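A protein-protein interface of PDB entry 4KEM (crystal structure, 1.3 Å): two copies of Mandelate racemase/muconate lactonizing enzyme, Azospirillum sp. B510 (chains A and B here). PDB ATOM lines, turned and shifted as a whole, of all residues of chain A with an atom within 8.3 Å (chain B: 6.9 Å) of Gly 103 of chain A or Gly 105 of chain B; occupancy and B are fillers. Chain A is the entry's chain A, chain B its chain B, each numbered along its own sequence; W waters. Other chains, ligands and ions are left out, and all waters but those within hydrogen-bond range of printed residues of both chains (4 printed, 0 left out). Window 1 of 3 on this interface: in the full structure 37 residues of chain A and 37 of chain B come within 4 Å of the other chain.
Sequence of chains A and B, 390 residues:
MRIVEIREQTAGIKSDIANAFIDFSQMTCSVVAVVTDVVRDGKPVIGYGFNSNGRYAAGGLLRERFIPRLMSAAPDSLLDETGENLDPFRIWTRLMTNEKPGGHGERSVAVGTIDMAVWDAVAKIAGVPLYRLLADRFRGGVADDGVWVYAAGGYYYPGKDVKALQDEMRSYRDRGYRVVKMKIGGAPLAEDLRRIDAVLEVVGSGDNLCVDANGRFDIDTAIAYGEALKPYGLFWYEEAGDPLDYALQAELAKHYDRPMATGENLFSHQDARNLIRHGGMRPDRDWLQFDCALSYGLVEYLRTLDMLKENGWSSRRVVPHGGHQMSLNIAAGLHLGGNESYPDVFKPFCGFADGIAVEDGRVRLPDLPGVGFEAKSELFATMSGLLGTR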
ATOM      1  N   ARG A  55      37.775  27.525  16.038  1.00  0.00           N
ATOM      2  CA  ARG A  55      36.472  28.078  16.367  1.00  0.00           C
ATOM      3  C   ARG A  55      36.415  28.713  17.759  1.00  0.00           C
ATOM      4  O   ARG A  55      35.406  29.345  18.096  1.00  0.00           O
ATOM      5  CB  ARG A  55      35.373  27.018  16.249  1.00  0.00           C
ATOM      6  CG  ARG A  55      35.221  26.329  14.879  1.00  0.00           C
ATOM      7  CD  ARG A  55      35.317  27.271  13.671  1.00  0.00           C
ATOM      8  NE  ARG A  55      34.265  28.265  13.632  1.00  0.00           N
ATOM      9  CZ  ARG A  55      33.821  28.832  12.516  1.00  0.00           C
ATOM     10  NH1 ARG A  55      34.271  28.473  11.329  1.00  0.00           N
ATOM     11  NH2 ARG A  55      32.901  29.786  12.592  1.00  0.00           N
ATOM     12  N   LEU A  61      28.638  29.221  26.643  1.00  0.00           N
ATOM     13  CA  LEU A  61      27.559  28.344  26.217  1.00  0.00           C
ATOM     14  C   LEU A  61      27.468  27.088  27.088  1.00  0.00           C
ATOM     15  O   LEU A  61      26.372  26.676  27.494  1.00  0.00           O
ATOM     16  CB  LEU A  61      27.729  27.980  24.750  1.00  0.00           C
ATOM     17  CG  LEU A  61      27.325  29.094  23.780  1.00  0.00           C
ATOM     18  CD1 LEU A  61      28.123  29.037  22.495  1.00  0.00           C
ATOM     19  CD2 LEU A  61      25.837  29.025  23.462  1.00  0.00           C
ATOM     20  N   ARG A  65      23.985  27.422  29.208  1.00  0.00           N
ATOM     21  CA  ARG A  65      22.903  26.680  28.573  1.00  0.00           C
ATOM     22  C   ARG A  65      23.015  25.164  28.745  1.00  0.00           C
ATOM     23  O   ARG A  65      22.111  24.504  29.271  1.00  0.00           O
ATOM     24  CB  ARG A  65      22.842  27.009  27.079  1.00  0.00           C
ATOM     25  CG  ARG A  65      22.601  28.495  26.771  1.00  0.00           C
ATOM     26  CD  ARG A  65      21.391  28.722  25.873  1.00  0.00           C
ATOM     27  NE  ARG A  65      21.542  28.237  24.498  1.00  0.00           N
ATOM     28  CZ  ARG A  65      22.135  28.904  23.512  1.00  0.00           C
ATOM     29  NH1 ARG A  65      22.161  28.389  22.300  1.00  0.00           N
ATOM     30  NH2 ARG A  65      22.706  30.090  23.713  1.00  0.00           N
ATOM     31  N   MET A  96      19.791  19.513  23.548  1.00  0.00           N
ATOM     32  CA  MET A  96      19.264  20.370  22.489  1.00  0.00           C
ATOM     33  C   MET A  96      17.812  20.744  22.669  1.00  0.00           C
ATOM     34  O   MET A  96      17.201  21.377  21.795  1.00  0.00           O
ATOM     35  CB  MET A  96      19.475  19.713  21.136  1.00  0.00           C
ATOM     36  CG  MET A  96      20.944  19.706  20.756  1.00  0.00           C
ATOM     37  SD  MET A  96      21.681  21.357  20.589  1.00  0.00           S
ATOM     38  CE  MET A  96      20.809  21.891  19.119  1.00  0.00           C
ATOM     39  N   GLU A  99      16.243  24.497  21.864  1.00  0.00           N
ATOM     40  CA  GLU A  99      17.141  25.162  20.913  1.00  0.00           C
ATOM     41  C   GLU A  99      16.456  25.307  19.555  1.00  0.00           C
ATOM     42  O   GLU A  99      15.948  24.334  18.990  1.00  0.00           O
ATOM     43  CB  GLU A  99      18.422  24.363  20.771  1.00  0.00           C
ATOM     44  CG  GLU A  99      19.257  24.351  22.037  1.00  0.00           C
ATOM     45  CD  GLU A  99      19.954  25.655  22.329  1.00  0.00           C
ATOM     46  OE1 GLU A  99      20.358  26.368  21.379  1.00  0.00           O
ATOM     47  OE2 GLU A  99      20.144  25.954  23.526  1.00  0.00           O
ATOM     48  N   LYS A 100      16.397  26.535  19.045  1.00  0.00           N
ATOM     49  CA  LYS A 100      15.772  26.752  17.748  1.00  0.00           C
ATOM     50  C   LYS A 100      16.664  26.263  16.625  1.00  0.00           C
ATOM     51  O   LYS A 100      17.870  26.178  16.777  1.00  0.00           O
ATOM     52  CB  LYS A 100      15.419  28.238  17.534  1.00  0.00           C
ATOM     53  CG  LYS A 100      14.157  28.666  18.251  1.00  0.00           C
ATOM     54  CD  LYS A 100      13.906  30.158  18.075  1.00  0.00           C
ATOM     55  CE  LYS A 100      13.401  30.475  16.696  1.00  0.00           C
ATOM     56  NZ  LYS A 100      13.063  31.934  16.526  1.00  0.00           N
ATOM     57  N   PRO A 101      16.062  25.916  15.479  1.00  0.00           N
ATOM     58  CA  PRO A 101      16.823  25.444  14.325  1.00  0.00           C
ATOM     59  C   PRO A 101      17.590  26.557  13.622  1.00  0.00           C
ATOM     60  O   PRO A 101      17.326  27.729  13.893  1.00  0.00           O
ATOM     61  CB  PRO A 101      15.747  24.877  13.412  1.00  0.00           C
ATOM     62  CG  PRO A 101      14.539  25.671  13.734  1.00  0.00           C
ATOM     63  CD  PRO A 101      14.617  25.983  15.207  1.00  0.00           C
ATOM     64  N   GLY A 102      18.486  26.184  12.713  1.00  0.00           N
ATOM     65  CA  GLY A 102      19.400  27.136  12.099  1.00  0.00           C
ATOM     66  C   GLY A 102      20.449  27.565  13.109  1.00  0.00           C
ATOM     67  O   GLY A 102      20.449  27.136  14.261  1.00  0.00           O
ATOM     68  N   GLY A 103      21.364  28.434  12.694  1.00  0.00           N
ATOM     69  CA  GLY A 103      22.338  28.968  13.623  1.00  0.00           C
ATOM     70  C   GLY A 103      23.369  27.960  14.124  1.00  0.00           C
ATOM     71  O   GLY A 103      23.695  27.977  15.318  1.00  0.00           O
ATOM     72  N   HIS A 104      23.932  27.154  13.222  1.00  0.00           N
ATOM     73  CA  HIS A 104      24.846  26.089  13.616  1.00  0.00           C
ATOM     74  C   HIS A 104      26.276  26.601  13.663  1.00  0.00           C
ATOM     75  O   HIS A 104      27.069  26.426  12.729  1.00  0.00           O
ATOM     76  CB  HIS A 104      24.678  24.873  12.696  1.00  0.00           C
ATOM     77  CG  HIS A 104      23.281  24.355  12.681  1.00  0.00           C
ATOM     78  ND1 HIS A 104      22.599  24.036  13.835  1.00  0.00           N
ATOM     79  CD2 HIS A 104      22.426  24.125  11.657  1.00  0.00           C
ATOM     80  CE1 HIS A 104      21.380  23.653  13.520  1.00  0.00           C
ATOM     81  NE2 HIS A 104      21.254  23.674  12.205  1.00  0.00           N
ATOM     82  N   GLY A 105      26.592  27.215  14.795  1.00  0.00           N
ATOM     83  CA  GLY A 105      27.908  27.705  15.126  1.00  0.00           C
ATOM     84  C   GLY A 105      27.955  27.979  16.623  1.00  0.00           C
ATOM     85  O   GLY A 105      26.924  28.316  17.235  1.00  0.00           O
ATOM     86  N   GLU A 106      29.145  27.813  17.198  1.00  0.00           N
ATOM     87  CA  GLU A 106      29.442  28.038  18.618  1.00  0.00           C
ATOM     88  C   GLU A 106      28.747  27.033  19.554  1.00  0.00           C
ATOM     89  O   GLU A 106      29.423  26.292  20.265  1.00  0.00           O
ATOM     90  CB  GLU A 106      29.145  29.475  19.053  1.00  0.00           C
ATOM     91  CG  GLU A 106      29.681  30.571  18.114  1.00  0.00           C
ATOM     92  CD  GLU A 106      31.206  30.741  18.077  1.00  0.00           C
ATOM     93  OE1 GLU A 106      31.886  30.480  19.102  1.00  0.00           O
ATOM     94  OE2 GLU A 106      31.696  31.189  17.007  1.00  0.00           O
ATOM     95  N   ARG A 107      27.416  27.000  19.566  1.00  0.00           N
ATOM     96  CA  ARG A 107      26.720  25.986  20.366  1.00  0.00           C
ATOM     97  C   ARG A 107      27.034  24.579  19.827  1.00  0.00           C
ATOM     98  O   ARG A 107      27.000  23.603  20.583  1.00  0.00           O
ATOM     99  CB  ARG A 107      25.204  26.253  20.444  1.00  0.00           C
ATOM    100  CG  ARG A 107      24.498  26.155  19.106  1.00  0.00           C
ATOM    101  CD  ARG A 107      22.979  26.088  19.289  1.00  0.00           C
ATOM    102  NE  ARG A 107      22.331  25.709  18.040  1.00  0.00           N
ATOM    103  CZ  ARG A 107      21.044  25.861  17.761  1.00  0.00           C
ATOM    104  NH1 ARG A 107      20.214  26.432  18.627  1.00  0.00           N
ATOM    105  NH2 ARG A 107      20.610  25.506  16.548  1.00  0.00           N
ATOM    106  N   SER A 108      27.321  24.495  18.524  1.00  0.00           N
ATOM    107  CA  SER A 108      27.744  23.231  17.905  1.00  0.00           C
ATOM    108  C   SER A 108      29.057  22.717  18.507  1.00  0.00           C
ATOM    109  O   SER A 108      29.276  21.517  18.599  1.00  0.00           O
ATOM    110  CB  SER A 108      27.870  23.440  16.392  1.00  0.00           C
ATOM    111  OG  SER A 108      28.772  24.500  16.126  1.00  0.00           O
ATOM    112  N   PHE A 267      28.745  22.725  10.224  1.00  0.00           N
ATOM    113  CA  PHE A 267      28.650  22.218  11.602  1.00  0.00           C
ATOM    114  C   PHE A 267      27.332  21.502  11.930  1.00  0.00           C
ATOM    115  O   PHE A 267      26.981  21.357  13.089  1.00  0.00           O
ATOM    116  CB  PHE A 267      28.921  23.352  12.604  1.00  0.00           C
ATOM    117  CG  PHE A 267      30.229  24.052  12.385  1.00  0.00           C
ATOM    118  CD1 PHE A 267      31.403  23.333  12.382  1.00  0.00           C
ATOM    119  CD2 PHE A 267      30.287  25.428  12.187  1.00  0.00           C
ATOM    120  CE1 PHE A 267      32.610  23.976  12.181  1.00  0.00           C
ATOM    121  CE2 PHE A 267      31.492  26.074  11.966  1.00  0.00           C
ATOM    122  CZ  PHE A 267      32.661  25.341  11.962  1.00  0.00           C
ATOM    123  N   SER A 268      26.626  21.042  10.897  1.00  0.00           N
ATOM    124  CA  SER A 268      25.389  20.277  11.081  1.00  0.00           C
ATOM    125  C   SER A 268      25.155  19.380   9.875  1.00  0.00           C
ATOM    126  O   SER A 268      25.718  19.609   8.789  1.00  0.00           O
ATOM    127  CB  SER A 268      24.203  21.229  11.206  1.00  0.00           C
ATOM    128  OG  SER A 268      23.933  21.866   9.956  1.00  0.00           O
ATOM    129  N   ASP A 271      23.671  21.584   7.050  1.00  0.00           N
ATOM    130  CA  ASP A 271      24.653  22.313   6.260  1.00  0.00           C
ATOM    131  C   ASP A 271      25.462  21.372   5.357  1.00  0.00           C
ATOM    132  O   ASP A 271      25.725  21.687   4.202  1.00  0.00           O
ATOM    133  CB  ASP A 271      25.571  23.120   7.178  1.00  0.00           C
ATOM    134  CG  ASP A 271      24.852  24.282   7.859  1.00  0.00           C
ATOM    135  OD1 ASP A 271      24.272  25.136   7.130  1.00  0.00           O
ATOM    136  OD2 ASP A 271      24.862  24.336   9.125  1.00  0.00           O
ATOM    137  N   TYR A 296      28.224  19.389  16.930  1.00  0.00           N
ATOM    138  CA  TYR A 296      27.281  18.710  17.818  1.00  0.00           C
ATOM    139  C   TYR A 296      27.598  17.222  18.007  1.00  0.00           C
ATOM    140  O   TYR A 296      26.728  16.469  18.450  1.00  0.00           O
ATOM    141  CB  TYR A 296      25.807  18.861  17.382  1.00  0.00           C
ATOM    142  CG  TYR A 296      25.284  20.257  17.087  1.00  0.00           C
ATOM    143  CD1 TYR A 296      24.664  21.005  18.074  1.00  0.00           C
ATOM    144  CD2 TYR A 296      25.359  20.788  15.813  1.00  0.00           C
ATOM    145  CE1 TYR A 296      24.151  22.274  17.800  1.00  0.00           C
ATOM    146  CE2 TYR A 296      24.831  22.038  15.525  1.00  0.00           C
ATOM    147  CZ  TYR A 296      24.240  22.778  16.519  1.00  0.00           C
ATOM    148  OH  TYR A 296      23.716  24.015  16.244  1.00  0.00           O
ATOM    149  N   ARG B  55      17.030  33.135  20.465  1.00  0.00           N
ATOM    150  CA  ARG B  55      18.387  32.636  20.351  1.00  0.00           C
ATOM    151  C   ARG B  55      19.207  32.658  21.650  1.00  0.00           C
ATOM    152  O   ARG B  55      20.330  32.131  21.650  1.00  0.00           O
ATOM    153  CB  ARG B  55      19.157  33.410  19.280  1.00  0.00           C
ATOM    154  CG  ARG B  55      18.538  33.398  17.877  1.00  0.00           C
ATOM    155  CD  ARG B  55      17.979  32.066  17.400  1.00  0.00           C
ATOM    156  NE  ARG B  55      18.978  31.017  17.321  1.00  0.00           N
ATOM    157  CZ  ARG B  55      18.880  29.977  16.497  1.00  0.00           C
ATOM    158  NH1 ARG B  55      17.855  29.854  15.668  1.00  0.00           N
ATOM    159  NH2 ARG B  55      19.811  29.035  16.502  1.00  0.00           N
ATOM    160  N   LEU B  61      30.191  35.131  24.398  1.00  0.00           N
ATOM    161  CA  LEU B  61      30.864  35.585  23.191  1.00  0.00           C
ATOM    162  C   LEU B  61      31.276  37.051  23.305  1.00  0.00           C
ATOM    163  O   LEU B  61      32.371  37.448  22.917  1.00  0.00           O
ATOM    164  CB  LEU B  61      29.970  35.356  21.985  1.00  0.00           C
ATOM    165  CG  LEU B  61      30.035  33.873  21.613  1.00  0.00           C
ATOM    166  CD1 LEU B  61      28.706  33.363  21.122  1.00  0.00           C
ATOM    167  CD2 LEU B  61      31.149  33.611  20.595  1.00  0.00           C
ATOM    168  N   GLY B 102      31.846  30.500   7.855  1.00  0.00           N
ATOM    169  CA  GLY B 102      30.882  29.501   8.280  1.00  0.00           C
ATOM    170  C   GLY B 102      30.510  29.719   9.732  1.00  0.00           C
ATOM    171  O   GLY B 102      31.011  30.612  10.427  1.00  0.00           O
ATOM    172  N   GLY B 103      29.633  28.868  10.241  1.00  0.00           N
ATOM    173  CA  GLY B 103      29.309  28.885  11.660  1.00  0.00           C
ATOM    174  C   GLY B 103      28.536  30.127  12.114  1.00  0.00           C
ATOM    175  O   GLY B 103      28.835  30.697  13.172  1.00  0.00           O
ATOM    176  N   HIS B 104      27.533  30.536  11.344  1.00  0.00           N
ATOM    177  CA  HIS B 104      26.797  31.769  11.606  1.00  0.00           C
ATOM    178  C   HIS B 104      25.663  31.513  12.603  1.00  0.00           C
ATOM    179  O   HIS B 104      24.500  31.347  12.234  1.00  0.00           O
ATOM    180  CB  HIS B 104      26.326  32.412  10.292  1.00  0.00           C
ATOM    181  CG  HIS B 104      27.455  32.703   9.364  1.00  0.00           C
ATOM    182  ND1 HIS B 104      28.571  33.400   9.762  1.00  0.00           N
ATOM    183  CD2 HIS B 104      27.657  32.356   8.074  1.00  0.00           C
ATOM    184  CE1 HIS B 104      29.420  33.457   8.758  1.00  0.00           C
ATOM    185  NE2 HIS B 104      28.885  32.847   7.716  1.00  0.00           N
ATOM    186  N   GLY B 105      26.028  31.486  13.886  1.00  0.00           N
ATOM    187  CA  GLY B 105      25.114  31.359  15.002  1.00  0.00           C
ATOM    188  C   GLY B 105      25.848  31.790  16.260  1.00  0.00           C
ATOM    189  O   GLY B 105      27.073  31.641  16.360  1.00  0.00           O
ATOM    190  N   GLU B 106      25.085  32.337  17.202  1.00  0.00           N
ATOM    191  CA  GLU B 106      25.559  32.805  18.507  1.00  0.00           C
ATOM    192  C   GLU B 106      26.495  34.021  18.398  1.00  0.00           C
ATOM    193  O   GLU B 106      26.167  35.089  18.914  1.00  0.00           O
ATOM    194  CB  GLU B 106      26.219  31.688  19.320  1.00  0.00           C
ATOM    195  CG  GLU B 106      25.416  30.372  19.385  1.00  0.00           C
ATOM    196  CD  GLU B 106      24.107  30.409  20.185  1.00  0.00           C
ATOM    197  OE1 GLU B 106      23.975  31.159  21.174  1.00  0.00           O
ATOM    198  OE2 GLU B 106      23.227  29.591  19.831  1.00  0.00           O
ATOM    199  N   ARG B 107      27.642  33.876  17.734  1.00  0.00           N
ATOM    200  CA  ARG B 107      28.503  35.047  17.528  1.00  0.00           C
ATOM    201  C   ARG B 107      27.789  36.090  16.646  1.00  0.00           C
ATOM    202  O   ARG B 107      28.085  37.269  16.733  1.00  0.00           O
ATOM    203  CB  ARG B 107      29.870  34.676  16.929  1.00  0.00           C
ATOM    204  CG  ARG B 107      29.807  34.121  15.554  1.00  0.00           C
ATOM    205  CD  ARG B 107      31.182  34.041  14.930  1.00  0.00           C
ATOM    206  NE  ARG B 107      31.076  33.730  13.512  1.00  0.00           N
ATOM    207  CZ  ARG B 107      32.071  33.303  12.733  1.00  0.00           C
ATOM    208  NH1 ARG B 107      33.305  33.118  13.203  1.00  0.00           N
ATOM    209  NH2 ARG B 107      31.805  33.033  11.448  1.00  0.00           N
ATOM    210  N   SER B 108      26.900  35.639  15.763  1.00  0.00           N
ATOM    211  CA  SER B 108      26.073  36.541  14.961  1.00  0.00           C
ATOM    212  C   SER B 108      25.178  37.432  15.825  1.00  0.00           C
ATOM    213  O   SER B 108      24.889  38.575  15.480  1.00  0.00           O
ATOM    214  CB  SER B 108      25.220  35.713  13.983  1.00  0.00           C
ATOM    215  OG  SER B 108      24.416  34.759  14.651  1.00  0.00           O
ATOM    216  N   VAL B 109      24.729  36.886  16.946  1.00  0.00           N
ATOM    217  CA  VAL B 109      23.912  37.594  17.924  1.00  0.00           C
ATOM    218  C   VAL B 109      24.766  38.589  18.704  1.00  0.00           C
ATOM    219  O   VAL B 109      24.353  39.723  18.908  1.00  0.00           O
ATOM    220  CB  VAL B 109      23.231  36.565  18.877  1.00  0.00           C
ATOM    221  CG1 VAL B 109      22.375  37.250  19.901  1.00  0.00           C
ATOM    222  CG2 VAL B 109      22.382  35.571  18.071  1.00  0.00           C
ATOM    223  N   PRO B 243      14.815  25.773   8.632  1.00  0.00           N
ATOM    224  CA  PRO B 243      15.218  26.999   7.932  1.00  0.00           C
ATOM    225  C   PRO B 243      16.309  26.799   6.906  1.00  0.00           C
ATOM    226  O   PRO B 243      16.428  27.586   5.975  1.00  0.00           O
ATOM    227  CB  PRO B 243      15.767  27.878   9.060  1.00  0.00           C
ATOM    228  CG  PRO B 243      16.020  26.940  10.217  1.00  0.00           C
ATOM    229  CD  PRO B 243      14.954  25.927  10.088  1.00  0.00           C
ATOM    230  N   LEU B 244      17.134  25.773   7.084  1.00  0.00           N
ATOM    231  CA  LEU B 244      18.234  25.503   6.156  1.00  0.00           C
ATOM    232  C   LEU B 244      17.891  24.466   5.065  1.00  0.00           C
ATOM    233  O   LEU B 244      18.709  24.209   4.186  1.00  0.00           O
ATOM    234  CB  LEU B 244      19.465  25.034   6.948  1.00  0.00           C
ATOM    235  CG  LEU B 244      20.139  26.051   7.866  1.00  0.00           C
ATOM    236  CD1 LEU B 244      21.000  25.424   8.934  1.00  0.00           C
ATOM    237  CD2 LEU B 244      20.951  27.039   7.013  1.00  0.00           C
ATOM    238  N   ASN B 265      15.746  32.602  10.887  1.00  0.00           N
ATOM    239  CA  ASN B 265      16.790  31.772  11.463  1.00  0.00           C
ATOM    240  C   ASN B 265      17.973  31.615  10.527  1.00  0.00           C
ATOM    241  O   ASN B 265      18.758  30.696  10.705  1.00  0.00           O
ATOM    242  CB  ASN B 265      16.230  30.400  11.868  1.00  0.00           C
ATOM    243  CG  ASN B 265      15.339  30.473  13.115  1.00  0.00           C
ATOM    244  OD1 ASN B 265      15.721  31.053  14.148  1.00  0.00           O
ATOM    245  ND2 ASN B 265      14.174  29.870  13.041  1.00  0.00           N
ATOM    246  N   LEU B 266      18.108  32.520   9.549  1.00  0.00           N
ATOM    247  CA  LEU B 266      19.303  32.627   8.709  1.00  0.00           C
ATOM    248  C   LEU B 266      20.051  33.894   9.127  1.00  0.00           C
ATOM    249  O   LEU B 266      19.475  34.983   9.088  1.00  0.00           O
ATOM    250  CB  LEU B 266      18.921  32.657   7.231  1.00  0.00           C
ATOM    251  CG  LEU B 266      18.098  31.452   6.757  1.00  0.00           C
ATOM    252  CD1 LEU B 266      17.719  31.583   5.290  1.00  0.00           C
ATOM    253  CD2 LEU B 266      18.791  30.115   7.005  1.00  0.00           C
ATOM    254  N   PHE B 267      21.319  33.762   9.506  1.00  0.00           N
ATOM    255  CA  PHE B 267      22.011  34.800  10.285  1.00  0.00           C
ATOM    256  C   PHE B 267      23.228  35.405   9.544  1.00  0.00           C
ATOM    257  O   PHE B 267      24.105  35.992  10.173  1.00  0.00           O
ATOM    258  CB  PHE B 267      22.417  34.262  11.669  1.00  0.00           C
ATOM    259  CG  PHE B 267      21.269  33.713  12.482  1.00  0.00           C
ATOM    260  CD1 PHE B 267      20.172  34.494  12.765  1.00  0.00           C
ATOM    261  CD2 PHE B 267      21.293  32.405  12.959  1.00  0.00           C
ATOM    262  CE1 PHE B 267      19.128  33.995  13.516  1.00  0.00           C
ATOM    263  CE2 PHE B 267      20.246  31.880  13.695  1.00  0.00           C
ATOM    264  CZ  PHE B 267      19.156  32.684  13.964  1.00  0.00           C
ATOM    265  N   ASP B 271      23.976  32.777   4.088  1.00  0.00           N
ATOM    266  CA  ASP B 271      22.837  31.889   4.315  1.00  0.00           C
ATOM    267  C   ASP B 271      21.577  32.452   3.623  1.00  0.00           C
ATOM    268  O   ASP B 271      20.816  31.702   3.024  1.00  0.00           O
ATOM    269  CB  ASP B 271      22.588  31.689   5.814  1.00  0.00           C
ATOM    270  CG  ASP B 271      23.682  30.883   6.496  1.00  0.00           C
ATOM    271  OD1 ASP B 271      23.948  29.725   6.081  1.00  0.00           O
ATOM    272  OD2 ASP B 271      24.296  31.415   7.452  1.00  0.00           O
ATOM    273  N   LEU B 294      20.240  39.483  15.126  1.00  0.00           N
ATOM    274  CA  LEU B 294      20.723  38.110  15.263  1.00  0.00           C
ATOM    275  C   LEU B 294      21.745  37.748  14.195  1.00  0.00           C
ATOM    276  O   LEU B 294      22.287  36.642  14.211  1.00  0.00           O
ATOM    277  CB  LEU B 294      19.539  37.134  15.149  1.00  0.00           C
ATOM    278  CG  LEU B 294      18.337  37.362  16.068  1.00  0.00           C
ATOM    279  CD1 LEU B 294      17.192  36.417  15.746  1.00  0.00           C
ATOM    280  CD2 LEU B 294      18.762  37.231  17.515  1.00  0.00           C
ATOM    281  N   TYR B 296      24.662  39.620  12.790  1.00  0.00           N
ATOM    282  CA  TYR B 296      25.840  40.494  12.679  1.00  0.00           C
ATOM    283  C   TYR B 296      25.488  41.937  12.334  1.00  0.00           C
ATOM    284  O   TYR B 296      26.349  42.686  11.908  1.00  0.00           O
ATOM    285  CB  TYR B 296      26.896  39.978  11.666  1.00  0.00           C
ATOM    286  CG  TYR B 296      27.383  38.552  11.819  1.00  0.00           C
ATOM    287  CD1 TYR B 296      28.481  38.249  12.608  1.00  0.00           C
ATOM    288  CD2 TYR B 296      26.761  37.527  11.134  1.00  0.00           C
ATOM    289  CE1 TYR B 296      28.962  36.932  12.708  1.00  0.00           C
ATOM    290  CE2 TYR B 296      27.240  36.212  11.230  1.00  0.00           C
ATOM    291  CZ  TYR B 296      28.322  35.934  12.016  1.00  0.00           C
ATOM    292  OH  TYR B 296      28.802  34.641  12.113  1.00  0.00           O
HETATM  293  O   HOH W   1      22.515  29.456  17.214  1.00  0.00           O
HETATM  294  O   HOH W   2      21.048  29.320   9.989  1.00  0.00           O
HETATM  295  O   HOH W   3      31.028  30.073  14.627  1.00  0.00           O
HETATM  296  O   HOH W   4      24.480  27.854   7.986  1.00  0.00           O
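Gly 105 of chain B touches three residues of chain A. Printed residues of chain B within 4 Å of His 104 of chain A: Gly 103 (3.5 Å) and Leu 244 (3.3 Å). Val 109 of chain B touches none of the printed residues of chain A. Tyr 296 of chain B touches none of the printed residues of chain A. The nearest printed residue of chain B that does not touch Gly 103 of chain A is Glu 106 of chain B (4.8 Å). The nearest printed residue of chain A that does not touch Leu 61 of chain B is Leu 61 of chain A (4.6 Å).
Water W3 lies within hydrogen-bond range of the backbone carbonyl oxygen (O) of Gly 103 of chain B, the side-chain carboxylate (OE2) of Glu 106 of chain A and the guanidinium group (NH2) of Arg 55 of chain A. Water W2 bridges O of Asn 265 of chain B and N of Gly 103 of chain A.
OE1 of Glu 99 of chain A is in salt-bridge range of NH1 of Arg 107 of chain A (2.8 Å). The backbone carbonyl oxygen (O) of Lys 100 of chain A is in hydrogen-bond range of the guanidinium group (NH2) of Arg 107 of chain A, at 2.8 Å.
Arg 55 of chain A touches Gly 103 of chain B. Leu 61 of chain A touches Glu 106 of chain B (CD2 to OE1, 3.6 Å). N of Gly 102 of chain A touches CG of Pro 243 of chain B, at 3.6 Å. O of Asn 265 of chain B touches CA of Gly 102 of chain A, at 3.9 Å. Gly 105 of chain A touches Gly 103 of chain B. Phe 267 of chain A touches Gly 103 of chain B (CE2 to CA, 3.6 Å).
Printed residues of chain B that touch a printed residue of chain A: Arg 55, Leu 61, Gly 102, Gly 103, His 104, Gly 105, Glu 106, Arg 107, Pro 243, Leu 244, Asn 265 and Phe 267. Of the 18 printed residues of chain A, 13 touch a printed residue of chain B. Hydrophobic or aromatic side chains of chain A that line the printed part of chain B: Leu 61, Pro 101, His 104 and Phe 267. Among the printed residues, 33 pairs touch across the chains. Among the printed residues, Asp or Glu carboxylates within 4 Å of a Lys or Arg side-chain nitrogen of the other chain: Arg 65 of chain A with Glu 106 of chain B (2.9 Å).
The guanidinium group of Arg 55 of chain A sits at hydrogen-bond distance from the backbone carbonyl oxygen of Gly 102 of chain B (3.0 Å). The guanidinium group (NH1) of Arg 65 of chain A lies within salt-bridge range of the side-chain carboxylate (OE2) of Glu 106 of chain B, 2.9 Å away. NH2 of Arg 55 of chain B is in hydrogen-bond range of O of Lys 100 of chain A, at 3.5 Å. NH1 of Arg 55 of chain B lies within hydrogen-bond range of O of Pro 101 of chain A, at 2.8 Å. The guanidinium group (NH2) of Arg 55 of chain B is in hydrogen-bond range of the backbone carbonyl oxygen (O) of Gly 102 of chain A (3.0 Å). NH1 of Arg 107 of chain B sits close to NH2 of Arg 55 of chain A, 3.4 Å away. The backbone carbonyl oxygen of Gly 105 of chain A lies close to the backbone carbonyl oxygen of Gly 105 of chain B, at 3.4 Å. NH1 of Arg 107 of chain A sits close to NH2 of Arg 55 of chain B, 3.4 Å away.
Gly 103 of chain A touches His 104 of chain B, and with the chains exchanged His 104 of chain A touches Gly 103 of chain B. Gly 103 of chain A touches Gly 105 of chain B, and with the chains exchanged Gly 105 of chain A touches Gly 103 of chain B.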
